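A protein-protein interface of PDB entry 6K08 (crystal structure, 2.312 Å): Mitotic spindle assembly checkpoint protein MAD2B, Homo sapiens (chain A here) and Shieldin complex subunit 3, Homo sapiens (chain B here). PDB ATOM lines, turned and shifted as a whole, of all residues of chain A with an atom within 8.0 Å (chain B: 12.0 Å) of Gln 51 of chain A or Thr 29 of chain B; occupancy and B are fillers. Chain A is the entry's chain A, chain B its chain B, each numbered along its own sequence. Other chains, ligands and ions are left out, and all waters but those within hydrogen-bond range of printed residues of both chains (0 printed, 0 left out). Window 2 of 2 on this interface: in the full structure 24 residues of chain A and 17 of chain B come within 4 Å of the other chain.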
ATOM      1  N   HIS A  36      12.294 -26.396 -24.887  1.00  0.00           N
ATOM      2  CA  HIS A  36      13.337 -25.382 -25.020  1.00  0.00           C
ATOM      3  C   HIS A  36      14.461 -25.864 -25.926  1.00  0.00           C
ATOM      4  O   HIS A  36      14.893 -25.152 -26.839  1.00  0.00           O
ATOM      5  CB  HIS A  36      13.892 -25.021 -23.641  1.00  0.00           C
ATOM      6  CG  HIS A  36      13.088 -23.992 -22.910  1.00  0.00           C
ATOM      7  ND1 HIS A  36      13.504 -22.685 -22.772  1.00  0.00           N
ATOM      8  CD2 HIS A  36      11.901 -24.078 -22.267  1.00  0.00           C
ATOM      9  CE1 HIS A  36      12.605 -22.009 -22.080  1.00  0.00           C
ATOM     10  NE2 HIS A  36      11.621 -22.832 -21.761  1.00  0.00           N
ATOM     11  N   TYR A  40      15.792 -24.836 -29.759  1.00  0.00           N
ATOM     12  CA  TYR A  40      17.182 -24.450 -29.977  1.00  0.00           C
ATOM     13  C   TYR A  40      17.799 -25.224 -31.137  1.00  0.00           C
ATOM     14  O   TYR A  40      18.235 -24.632 -32.131  1.00  0.00           O
ATOM     15  CB  TYR A  40      17.998 -24.665 -28.699  1.00  0.00           C
ATOM     16  CG  TYR A  40      19.484 -24.457 -28.892  1.00  0.00           C
ATOM     17  CD1 TYR A  40      20.027 -23.179 -28.918  1.00  0.00           C
ATOM     18  CD2 TYR A  40      20.343 -25.537 -29.060  1.00  0.00           C
ATOM     19  CE1 TYR A  40      21.382 -22.982 -29.098  1.00  0.00           C
ATOM     20  CE2 TYR A  40      21.699 -25.349 -29.242  1.00  0.00           C
ATOM     21  CZ  TYR A  40      22.214 -24.070 -29.260  1.00  0.00           C
ATOM     22  OH  TYR A  40      23.565 -23.879 -29.439  1.00  0.00           O
ATOM     23  N   PRO A  46      16.032 -17.234 -32.523  1.00  0.00           N
ATOM     24  CA  PRO A  46      17.460 -16.900 -32.605  1.00  0.00           C
ATOM     25  C   PRO A  46      18.260 -17.499 -31.457  1.00  0.00           C
ATOM     26  O   PRO A  46      17.761 -17.681 -30.345  1.00  0.00           O
ATOM     27  CB  PRO A  46      17.471 -15.368 -32.550  1.00  0.00           C
ATOM     28  CG  PRO A  46      16.132 -14.967 -33.049  1.00  0.00           C
ATOM     29  CD  PRO A  46      15.186 -16.028 -32.570  1.00  0.00           C
ATOM     30  N   VAL A  47      19.529 -17.801 -31.748  1.00  0.00           N
ATOM     31  CA  VAL A  47      20.404 -18.418 -30.758  1.00  0.00           C
ATOM     32  C   VAL A  47      20.700 -17.482 -29.592  1.00  0.00           C
ATOM     33  O   VAL A  47      21.088 -17.946 -28.513  1.00  0.00           O
ATOM     34  CB  VAL A  47      21.710 -18.881 -31.432  1.00  0.00           C
ATOM     35  CG1 VAL A  47      22.610 -17.690 -31.735  1.00  0.00           C
ATOM     36  CG2 VAL A  47      22.433 -19.904 -30.567  1.00  0.00           C
ATOM     37  N   GLY A  48      20.512 -16.172 -29.771  1.00  0.00           N
ATOM     38  CA  GLY A  48      20.868 -15.230 -28.723  1.00  0.00           C
ATOM     39  C   GLY A  48      20.007 -15.340 -27.482  1.00  0.00           C
ATOM     40  O   GLY A  48      20.467 -15.037 -26.378  1.00  0.00           O
ATOM     41  N   ILE A  49      18.753 -15.775 -27.638  1.00  0.00           N
ATOM     42  CA  ILE A  49      17.846 -15.874 -26.494  1.00  0.00           C
ATOM     43  C   ILE A  49      18.135 -17.069 -25.602  1.00  0.00           C
ATOM     44  O   ILE A  49      17.549 -17.168 -24.517  1.00  0.00           O
ATOM     45  CB  ILE A  49      16.372 -15.959 -26.934  1.00  0.00           C
ATOM     46  CG1 ILE A  49      16.088 -17.302 -27.606  1.00  0.00           C
ATOM     47  CG2 ILE A  49      16.018 -14.809 -27.860  1.00  0.00           C
ATOM     48  CD1 ILE A  49      14.614 -17.605 -27.753  1.00  0.00           C
ATOM     49  N   PHE A  50      19.019 -17.968 -26.018  1.00  0.00           N
ATOM     50  CA  PHE A  50      19.265 -19.206 -25.296  1.00  0.00           C
ATOM     51  C   PHE A  50      20.520 -19.106 -24.439  1.00  0.00           C
ATOM     52  O   PHE A  50      21.498 -18.444 -24.798  1.00  0.00           O
ATOM     53  CB  PHE A  50      19.389 -20.382 -26.262  1.00  0.00           C
ATOM     54  CG  PHE A  50      18.088 -20.781 -26.888  1.00  0.00           C
ATOM     55  CD1 PHE A  50      17.170 -21.538 -26.182  1.00  0.00           C
ATOM     56  CD2 PHE A  50      17.775 -20.388 -28.179  1.00  0.00           C
ATOM     57  CE1 PHE A  50      15.968 -21.901 -26.751  1.00  0.00           C
ATOM     58  CE2 PHE A  50      16.574 -20.749 -28.755  1.00  0.00           C
ATOM     59  CZ  PHE A  50      15.668 -21.507 -28.039  1.00  0.00           C
ATOM     60  N   GLN A  51      20.472 -19.787 -23.297  1.00  0.00           N
ATOM     61  CA  GLN A  51      21.571 -19.863 -22.350  1.00  0.00           C
ATOM     62  C   GLN A  51      21.929 -21.320 -22.095  1.00  0.00           C
ATOM     63  O   GLN A  51      21.047 -22.170 -21.925  1.00  0.00           O
ATOM     64  CB  GLN A  51      21.204 -19.167 -21.034  1.00  0.00           C
ATOM     65  CG  GLN A  51      22.205 -19.360 -19.911  1.00  0.00           C
ATOM     66  CD  GLN A  51      22.341 -18.128 -19.042  1.00  0.00           C
ATOM     67  OE1 GLN A  51      21.408 -17.748 -18.334  1.00  0.00           O
ATOM     68  NE2 GLN A  51      23.503 -17.489 -19.101  1.00  0.00           N
ATOM     69  N   LYS A  52      23.226 -21.605 -22.083  1.00  0.00           N
ATOM     70  CA  LYS A  52      23.712 -22.949 -21.800  1.00  0.00           C
ATOM     71  C   LYS A  52      23.615 -23.230 -20.308  1.00  0.00           C
ATOM     72  O   LYS A  52      24.225 -22.527 -19.491  1.00  0.00           O
ATOM     73  CB  LYS A  52      25.155 -23.107 -22.274  1.00  0.00           C
ATOM     74  CG  LYS A  52      25.275 -23.311 -23.764  1.00  0.00           C
ATOM     75  CD  LYS A  52      26.360 -22.451 -24.372  1.00  0.00           C
ATOM     76  CE  LYS A  52      26.546 -22.809 -25.839  1.00  0.00           C
ATOM     77  NZ  LYS A  52      25.996 -21.791 -26.783  1.00  0.00           N
ATOM     78  N   ARG A  53      22.865 -24.271 -19.956  1.00  0.00           N
ATOM     79  CA  ARG A  53      22.703 -24.697 -18.576  1.00  0.00           C
ATOM     80  C   ARG A  53      22.857 -26.209 -18.503  1.00  0.00           C
ATOM     81  O   ARG A  53      23.007 -26.888 -19.522  1.00  0.00           O
ATOM     82  CB  ARG A  53      21.342 -24.263 -18.011  1.00  0.00           C
ATOM     83  CG  ARG A  53      21.068 -22.772 -18.097  1.00  0.00           C
ATOM     84  CD  ARG A  53      20.205 -22.309 -16.933  1.00  0.00           C
ATOM     85  NE  ARG A  53      18.945 -21.733 -17.392  1.00  0.00           N
ATOM     86  CZ  ARG A  53      18.714 -20.428 -17.497  1.00  0.00           C
ATOM     87  NH1 ARG A  53      19.659 -19.557 -17.173  1.00  0.00           N
ATOM     88  NH2 ARG A  53      17.536 -19.995 -17.925  1.00  0.00           N
ATOM     89  N   LYS A  54      22.809 -26.741 -17.284  1.00  0.00           N
ATOM     90  CA  LYS A  54      22.838 -28.176 -17.050  1.00  0.00           C
ATOM     91  C   LYS A  54      21.552 -28.599 -16.358  1.00  0.00           C
ATOM     92  O   LYS A  54      21.195 -28.052 -15.308  1.00  0.00           O
ATOM     93  CB  LYS A  54      24.048 -28.585 -16.201  1.00  0.00           C
ATOM     94  CG  LYS A  54      25.396 -28.253 -16.818  1.00  0.00           C
ATOM     95  CD  LYS A  54      25.845 -29.342 -17.778  1.00  0.00           C
ATOM     96  CE  LYS A  54      26.822 -28.799 -18.808  1.00  0.00           C
ATOM     97  NZ  LYS A  54      26.203 -27.746 -19.660  1.00  0.00           N
ATOM     98  N   PRO A  59      24.208 -31.184 -20.721  1.00  0.00           N
ATOM     99  CA  PRO A  59      24.072 -29.819 -21.262  1.00  0.00           C
ATOM    100  C   PRO A  59      22.736 -29.607 -21.967  1.00  0.00           C
ATOM    101  O   PRO A  59      22.306 -30.431 -22.775  1.00  0.00           O
ATOM    102  CB  PRO A  59      25.245 -29.710 -22.243  1.00  0.00           C
ATOM    103  CG  PRO A  59      25.605 -31.131 -22.574  1.00  0.00           C
ATOM    104  CD  PRO A  59      25.348 -31.902 -21.318  1.00  0.00           C
ATOM    105  N   VAL A  60      22.083 -28.480 -21.656  1.00  0.00           N
ATOM    106  CA  VAL A  60      20.812 -28.093 -22.264  1.00  0.00           C
ATOM    107  C   VAL A  60      20.855 -26.609 -22.615  1.00  0.00           C
ATOM    108  O   VAL A  60      21.799 -25.891 -22.279  1.00  0.00           O
ATOM    109  CB  VAL A  60      19.600 -28.382 -21.349  1.00  0.00           C
ATOM    110  CG1 VAL A  60      19.601 -29.828 -20.884  1.00  0.00           C
ATOM    111  CG2 VAL A  60      19.591 -27.434 -20.159  1.00  0.00           C
ATOM    112  N   GLN A  61      19.804 -26.150 -23.298  1.00  0.00           N
ATOM    113  CA  GLN A  61      19.691 -24.763 -23.745  1.00  0.00           C
ATOM    114  C   GLN A  61      18.319 -24.232 -23.351  1.00  0.00           C
ATOM    115  O   GLN A  61      17.295 -24.719 -23.845  1.00  0.00           O
ATOM    116  CB  GLN A  61      19.897 -24.652 -25.256  1.00  0.00           C
ATOM    117  CG  GLN A  61      21.227 -25.200 -25.750  1.00  0.00           C
ATOM    118  CD  GLN A  61      22.314 -24.147 -25.780  1.00  0.00           C
ATOM    119  OE1 GLN A  61      22.065 -22.977 -25.493  1.00  0.00           O
ATOM    120  NE2 GLN A  61      23.525 -24.554 -26.144  1.00  0.00           N
ATOM    121  N   MET A  62      18.297 -23.235 -22.472  1.00  0.00           N
ATOM    122  CA  MET A  62      17.064 -22.597 -22.035  1.00  0.00           C
ATOM    123  C   MET A  62      16.983 -21.188 -22.602  1.00  0.00           C
ATOM    124  O   MET A  62      17.970 -20.444 -22.587  1.00  0.00           O
ATOM    125  CB  MET A  62      16.975 -22.552 -20.506  1.00  0.00           C
ATOM    126  CG  MET A  62      17.240 -23.883 -19.826  1.00  0.00           C
ATOM    127  SD  MET A  62      15.975 -25.117 -20.181  1.00  0.00           S
ATOM    128  CE  MET A  62      14.564 -24.425 -19.322  1.00  0.00           C
ATOM    129  N   SER A  63      15.809 -20.830 -23.110  1.00  0.00           N
ATOM    130  CA  SER A  63      15.590 -19.473 -23.584  1.00  0.00           C
ATOM    131  C   SER A  63      15.432 -18.530 -22.402  1.00  0.00           C
ATOM    132  O   SER A  63      14.856 -18.890 -21.372  1.00  0.00           O
ATOM    133  CB  SER A  63      14.350 -19.408 -24.477  1.00  0.00           C
ATOM    134  OG  SER A  63      13.204 -19.050 -23.725  1.00  0.00           O
ATOM    135  N   CYS A  64      15.962 -17.319 -22.549  1.00  0.00           N
ATOM    136  CA  CYS A  64      15.780 -16.268 -21.559  1.00  0.00           C
ATOM    137  C   CYS A  64      14.731 -15.252 -21.982  1.00  0.00           C
ATOM    138  O   CYS A  64      14.643 -14.178 -21.378  1.00  0.00           O
ATOM    139  CB  CYS A  64      17.109 -15.568 -21.276  1.00  0.00           C
ATOM    140  SG  CYS A  64      18.391 -16.666 -20.642  1.00  0.00           S
ATOM    141  N   HIS A  65      13.937 -15.560 -23.002  1.00  0.00           N
ATOM    142  CA  HIS A  65      12.869 -14.661 -23.409  1.00  0.00           C
ATOM    143  C   HIS A  65      11.695 -14.802 -22.448  1.00  0.00           C
ATOM    144  O   HIS A  65      11.124 -15.892 -22.341  1.00  0.00           O
ATOM    145  CB  HIS A  65      12.422 -14.954 -24.834  1.00  0.00           C
ATOM    146  CG  HIS A  65      11.569 -13.878 -25.428  1.00  0.00           C
ATOM    147  ND1 HIS A  65      10.216 -13.780 -25.182  1.00  0.00           N
ATOM    148  CD2 HIS A  65      11.878 -12.843 -26.244  1.00  0.00           C
ATOM    149  CE1 HIS A  65       9.727 -12.738 -25.829  1.00  0.00           C
ATOM    150  NE2 HIS A  65      10.715 -12.152 -26.481  1.00  0.00           N
ATOM    151  N   ILE B  16       9.582 -13.410 -31.752  1.00  0.00           N
ATOM    152  CA  ILE B  16      10.694 -12.747 -31.088  1.00  0.00           C
ATOM    153  C   ILE B  16      11.561 -12.101 -32.156  1.00  0.00           C
ATOM    154  O   ILE B  16      12.270 -12.791 -32.899  1.00  0.00           O
ATOM    155  CB  ILE B  16      11.500 -13.722 -30.229  1.00  0.00           C
ATOM    156  CG1 ILE B  16      10.589 -14.367 -29.191  1.00  0.00           C
ATOM    157  CG2 ILE B  16      12.669 -13.007 -29.576  1.00  0.00           C
ATOM    158  CD1 ILE B  16      11.189 -15.562 -28.520  1.00  0.00           C
ATOM    159  N   GLU B  18      14.636 -10.054 -33.907  1.00  0.00           N
ATOM    160  CA  GLU B  18      16.081 -10.088 -33.707  1.00  0.00           C
ATOM    161  C   GLU B  18      16.526  -9.024 -32.715  1.00  0.00           C
ATOM    162  O   GLU B  18      17.482  -9.238 -31.958  1.00  0.00           O
ATOM    163  CB  GLU B  18      16.804  -9.904 -35.040  1.00  0.00           C
ATOM    164  CG  GLU B  18      16.638 -11.064 -36.004  1.00  0.00           C
ATOM    165  CD  GLU B  18      17.878 -11.931 -36.089  1.00  0.00           C
ATOM    166  OE1 GLU B  18      18.825 -11.545 -36.805  1.00  0.00           O
ATOM    167  OE2 GLU B  18      17.903 -12.998 -35.440  1.00  0.00           O
ATOM    168  N   GLU B  19      15.847  -7.876 -32.705  1.00  0.00           N
ATOM    169  CA  GLU B  19      16.134  -6.843 -31.717  1.00  0.00           C
ATOM    170  C   GLU B  19      15.874  -7.352 -30.306  1.00  0.00           C
ATOM    171  O   GLU B  19      16.693  -7.159 -29.400  1.00  0.00           O
ATOM    172  CB  GLU B  19      15.290  -5.604 -32.003  1.00  0.00           C
ATOM    173  CG  GLU B  19      16.075  -4.316 -32.022  1.00  0.00           C
ATOM    174  CD  GLU B  19      15.185  -3.101 -31.926  1.00  0.00           C
ATOM    175  OE1 GLU B  19      13.983  -3.211 -32.251  1.00  0.00           O
ATOM    176  OE2 GLU B  19      15.691  -2.037 -31.521  1.00  0.00           O
ATOM    177  N   ALA B  20      14.725  -8.000 -30.100  1.00  0.00           N
ATOM    178  CA  ALA B  20      14.434  -8.595 -28.800  1.00  0.00           C
ATOM    179  C   ALA B  20      15.458  -9.665 -28.450  1.00  0.00           C
ATOM    180  O   ALA B  20      15.876  -9.778 -27.292  1.00  0.00           O
ATOM    181  CB  ALA B  20      13.021  -9.178 -28.793  1.00  0.00           C
ATOM    182  N   ALA B  21      15.881 -10.452 -29.442  1.00  0.00           N
ATOM    183  CA  ALA B  21      16.881 -11.485 -29.193  1.00  0.00           C
ATOM    184  C   ALA B  21      18.213 -10.876 -28.775  1.00  0.00           C
ATOM    185  O   ALA B  21      18.869 -11.375 -27.853  1.00  0.00           O
ATOM    186  CB  ALA B  21      17.055 -12.356 -30.436  1.00  0.00           C
ATOM    187  N   GLU B  22      18.633  -9.800 -29.445  1.00  0.00           N
ATOM    188  CA  GLU B  22      19.855  -9.114 -29.040  1.00  0.00           C
ATOM    189  C   GLU B  22      19.725  -8.562 -27.627  1.00  0.00           C
ATOM    190  O   GLU B  22      20.658  -8.668 -26.823  1.00  0.00           O
ATOM    191  CB  GLU B  22      20.184  -7.994 -30.026  1.00  0.00           C
ATOM    192  N   ASP B  23      18.565  -7.982 -27.305  1.00  0.00           N
ATOM    193  CA  ASP B  23      18.325  -7.498 -25.950  1.00  0.00           C
ATOM    194  C   ASP B  23      18.372  -8.638 -24.938  1.00  0.00           C
ATOM    195  O   ASP B  23      18.961  -8.498 -23.860  1.00  0.00           O
ATOM    196  CB  ASP B  23      16.977  -6.782 -25.883  1.00  0.00           C
ATOM    197  CG  ASP B  23      17.050  -5.341 -26.345  1.00  0.00           C
ATOM    198  OD1 ASP B  23      18.141  -4.895 -26.759  1.00  0.00           O
ATOM    199  OD2 ASP B  23      16.009  -4.653 -26.292  1.00  0.00           O
ATOM    200  N   VAL B  24      17.750  -9.775 -25.267  1.00  0.00           N
ATOM    201  CA  VAL B  24      17.772 -10.924 -24.364  1.00  0.00           C
ATOM    202  C   VAL B  24      19.195 -11.442 -24.200  1.00  0.00           C
ATOM    203  O   VAL B  24      19.625 -11.779 -23.089  1.00  0.00           O
ATOM    204  CB  VAL B  24      16.821 -12.025 -24.873  1.00  0.00           C
ATOM    205  CG1 VAL B  24      17.038 -13.313 -24.097  1.00  0.00           C
ATOM    206  CG2 VAL B  24      15.374 -11.580 -24.752  1.00  0.00           C
ATOM    207  N   LYS B  25      19.947 -11.511 -25.299  1.00  0.00           N
ATOM    208  CA  LYS B  25      21.352 -11.897 -25.213  1.00  0.00           C
ATOM    209  C   LYS B  25      22.152 -10.882 -24.406  1.00  0.00           C
ATOM    210  O   LYS B  25      23.077 -11.248 -23.671  1.00  0.00           O
ATOM    211  CB  LYS B  25      21.931 -12.052 -26.622  1.00  0.00           C
ATOM    212  CG  LYS B  25      23.447 -11.931 -26.714  1.00  0.00           C
ATOM    213  CD  LYS B  25      24.148 -13.116 -26.066  1.00  0.00           C
ATOM    214  CE  LYS B  25      25.660 -12.950 -26.103  1.00  0.00           C
ATOM    215  NZ  LYS B  25      26.358 -14.011 -25.324  1.00  0.00           N
ATOM    216  N   GLN B  26      21.793  -9.602 -24.511  1.00  0.00           N
ATOM    217  CA  GLN B  26      22.596  -8.542 -23.912  1.00  0.00           C
ATOM    218  C   GLN B  26      22.295  -8.336 -22.432  1.00  0.00           C
ATOM    219  O   GLN B  26      23.214  -8.050 -21.655  1.00  0.00           O
ATOM    220  CB  GLN B  26      22.373  -7.234 -24.675  1.00  0.00           C
ATOM    221  CG  GLN B  26      22.976  -6.003 -24.023  1.00  0.00           C
ATOM    222  CD  GLN B  26      24.327  -5.645 -24.603  1.00  0.00           C
ATOM    223  OE1 GLN B  26      25.084  -6.516 -25.028  1.00  0.00           O
ATOM    224  NE2 GLN B  26      24.636  -4.353 -24.628  1.00  0.00           N
ATOM    225  N   TYR B  27      21.035  -8.479 -22.016  1.00  0.00           N
ATOM    226  CA  TYR B  27      20.628  -8.085 -20.676  1.00  0.00           C
ATOM    227  C   TYR B  27      20.110  -9.220 -19.803  1.00  0.00           C
ATOM    228  O   TYR B  27      20.089  -9.064 -18.578  1.00  0.00           O
ATOM    229  CB  TYR B  27      19.553  -6.990 -20.751  1.00  0.00           C
ATOM    230  CG  TYR B  27      20.041  -5.726 -21.425  1.00  0.00           C
ATOM    231  CD1 TYR B  27      21.046  -4.955 -20.853  1.00  0.00           C
ATOM    232  CD2 TYR B  27      19.504  -5.308 -22.636  1.00  0.00           C
ATOM    233  CE1 TYR B  27      21.496  -3.802 -21.463  1.00  0.00           C
ATOM    234  CE2 TYR B  27      19.950  -4.155 -23.255  1.00  0.00           C
ATOM    235  CZ  TYR B  27      20.947  -3.406 -22.664  1.00  0.00           C
ATOM    236  OH  TYR B  27      21.395  -2.258 -23.275  1.00  0.00           O
ATOM    237  N   LEU B  28      19.691 -10.344 -20.384  1.00  0.00           N
ATOM    238  CA  LEU B  28      19.244 -11.499 -19.615  1.00  0.00           C
ATOM    239  C   LEU B  28      20.181 -12.689 -19.785  1.00  0.00           C
ATOM    240  O   LEU B  28      19.789 -13.832 -19.519  1.00  0.00           O
ATOM    241  CB  LEU B  28      17.813 -11.870 -20.003  1.00  0.00           C
ATOM    242  CG  LEU B  28      16.874 -10.671 -20.150  1.00  0.00           C
ATOM    243  CD1 LEU B  28      15.548 -11.091 -20.758  1.00  0.00           C
ATOM    244  CD2 LEU B  28      16.665  -9.989 -18.804  1.00  0.00           C
ATOM    245  N   THR B  29      21.417 -12.427 -20.208  1.00  0.00           N
ATOM    246  CA  THR B  29      22.436 -13.433 -20.500  1.00  0.00           C
ATOM    247  C   THR B  29      21.887 -14.551 -21.385  1.00  0.00           C
ATOM    248  O   THR B  29      21.765 -14.385 -22.600  1.00  0.00           O
ATOM    249  CB  THR B  29      23.027 -14.040 -19.212  1.00  0.00           C
ATOM    250  OG1 THR B  29      23.075 -13.038 -18.191  1.00  0.00           O
ATOM    251  CG2 THR B  29      24.450 -14.531 -19.475  1.00  0.00           C
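The side-chain sulfur (SG) of Cys 64 of chain A lies within hydrogen-bond range of the backbone carbonyl oxygen (O) of Leu 28 of chain B (3.4 Å).
The backbone carbonyl oxygen of Ile 49 of chain A lies within hydrogen-bond range of the backbone NH of Cys 64 of chain A.
The side-chain amide oxygen (OE1) of Gln 51 of chain A lies within hydrogen-bond range of the guanidinium group (NH1) of Arg 53 of chain A (2.8 Å).
The backbone carbonyl oxygen (O) of Met 62 of chain A is in hydrogen-bond range of the backbone NH (N) of Gln 51 of chain A.
O of Val 24 of chain B is in hydrogen-bond range of N of Thr 29 of chain B, 3.5 Å away.
Among the printed residues, pairs that only touch across the chains: Gln 51 of chain A with Thr 29 of chain B (3.1 Å), Gly 48 of chain A with Lys 25 of chain B (3.3 Å), His 65 of chain A with Ile 16 of chain B (3.4 Å), Pro 46 of chain A with Glu 18 of chain B (3.6 Å), Ile 49 of chain A with Val 24 of chain B (3.6 Å), Cys 64 of chain A with Val 24 of chain B (3.6 Å), Ile 49 of chain A with Ala 21 of chain B (3.7 Å), Pro 46 of chain A with Ala 21 of chain B (3.7 Å) and His 65 of chain A with Val 24 of chain B (3.98 Å).
Ile 49 of chain A touches just these residues of chain B: Ala 21 (3.7 Å) and Val 24 (3.6 Å).
No residue of chain B comes within 4 Å of Phe 50 of chain A.
No residue of chain B comes within 4 Å of Lys 52 of chain A.
Arg 53 of chain A touches none of the printed residues of chain B.
No residue of chain B comes within 4 Å of Gln 61 of chain A.
No residue of chain B comes within 4 Å of Ser 63 of chain A.
Cys 64 of chain A touches just these residues of chain B: Val 24 (3.6 Å) and Leu 28 (3.3 Å).
Printed residues of chain B within 4 Å of His 65 of chain A: Ile 16 (3.4 Å) and Val 24 (3.98 Å).
Of the printed residues of chain A, Glu 18 of chain B touches Pro 46 (3.6 Å).
Printed residues of chain B within 4 Å of Pro 46 of chain A: Glu 18 and Ala 21.
Of the printed residues of chain A, Leu 28 of chain B touches Cys 64.
His 36 of chain A touches none of the printed residues of chain B.
Ala 20 of chain B touches none of the printed residues of chain A.
The nearest residue of chain B that does not touch Gln 51 of chain A is Leu 28 of chain B (4.4 Å).
Of the 13 printed residues of chain B, 7 touch a printed residue of chain A.
Among the printed residues, no Asp or Glu carboxylate lies within 4 Å of a Lys or Arg side-chain nitrogen of the other chain.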
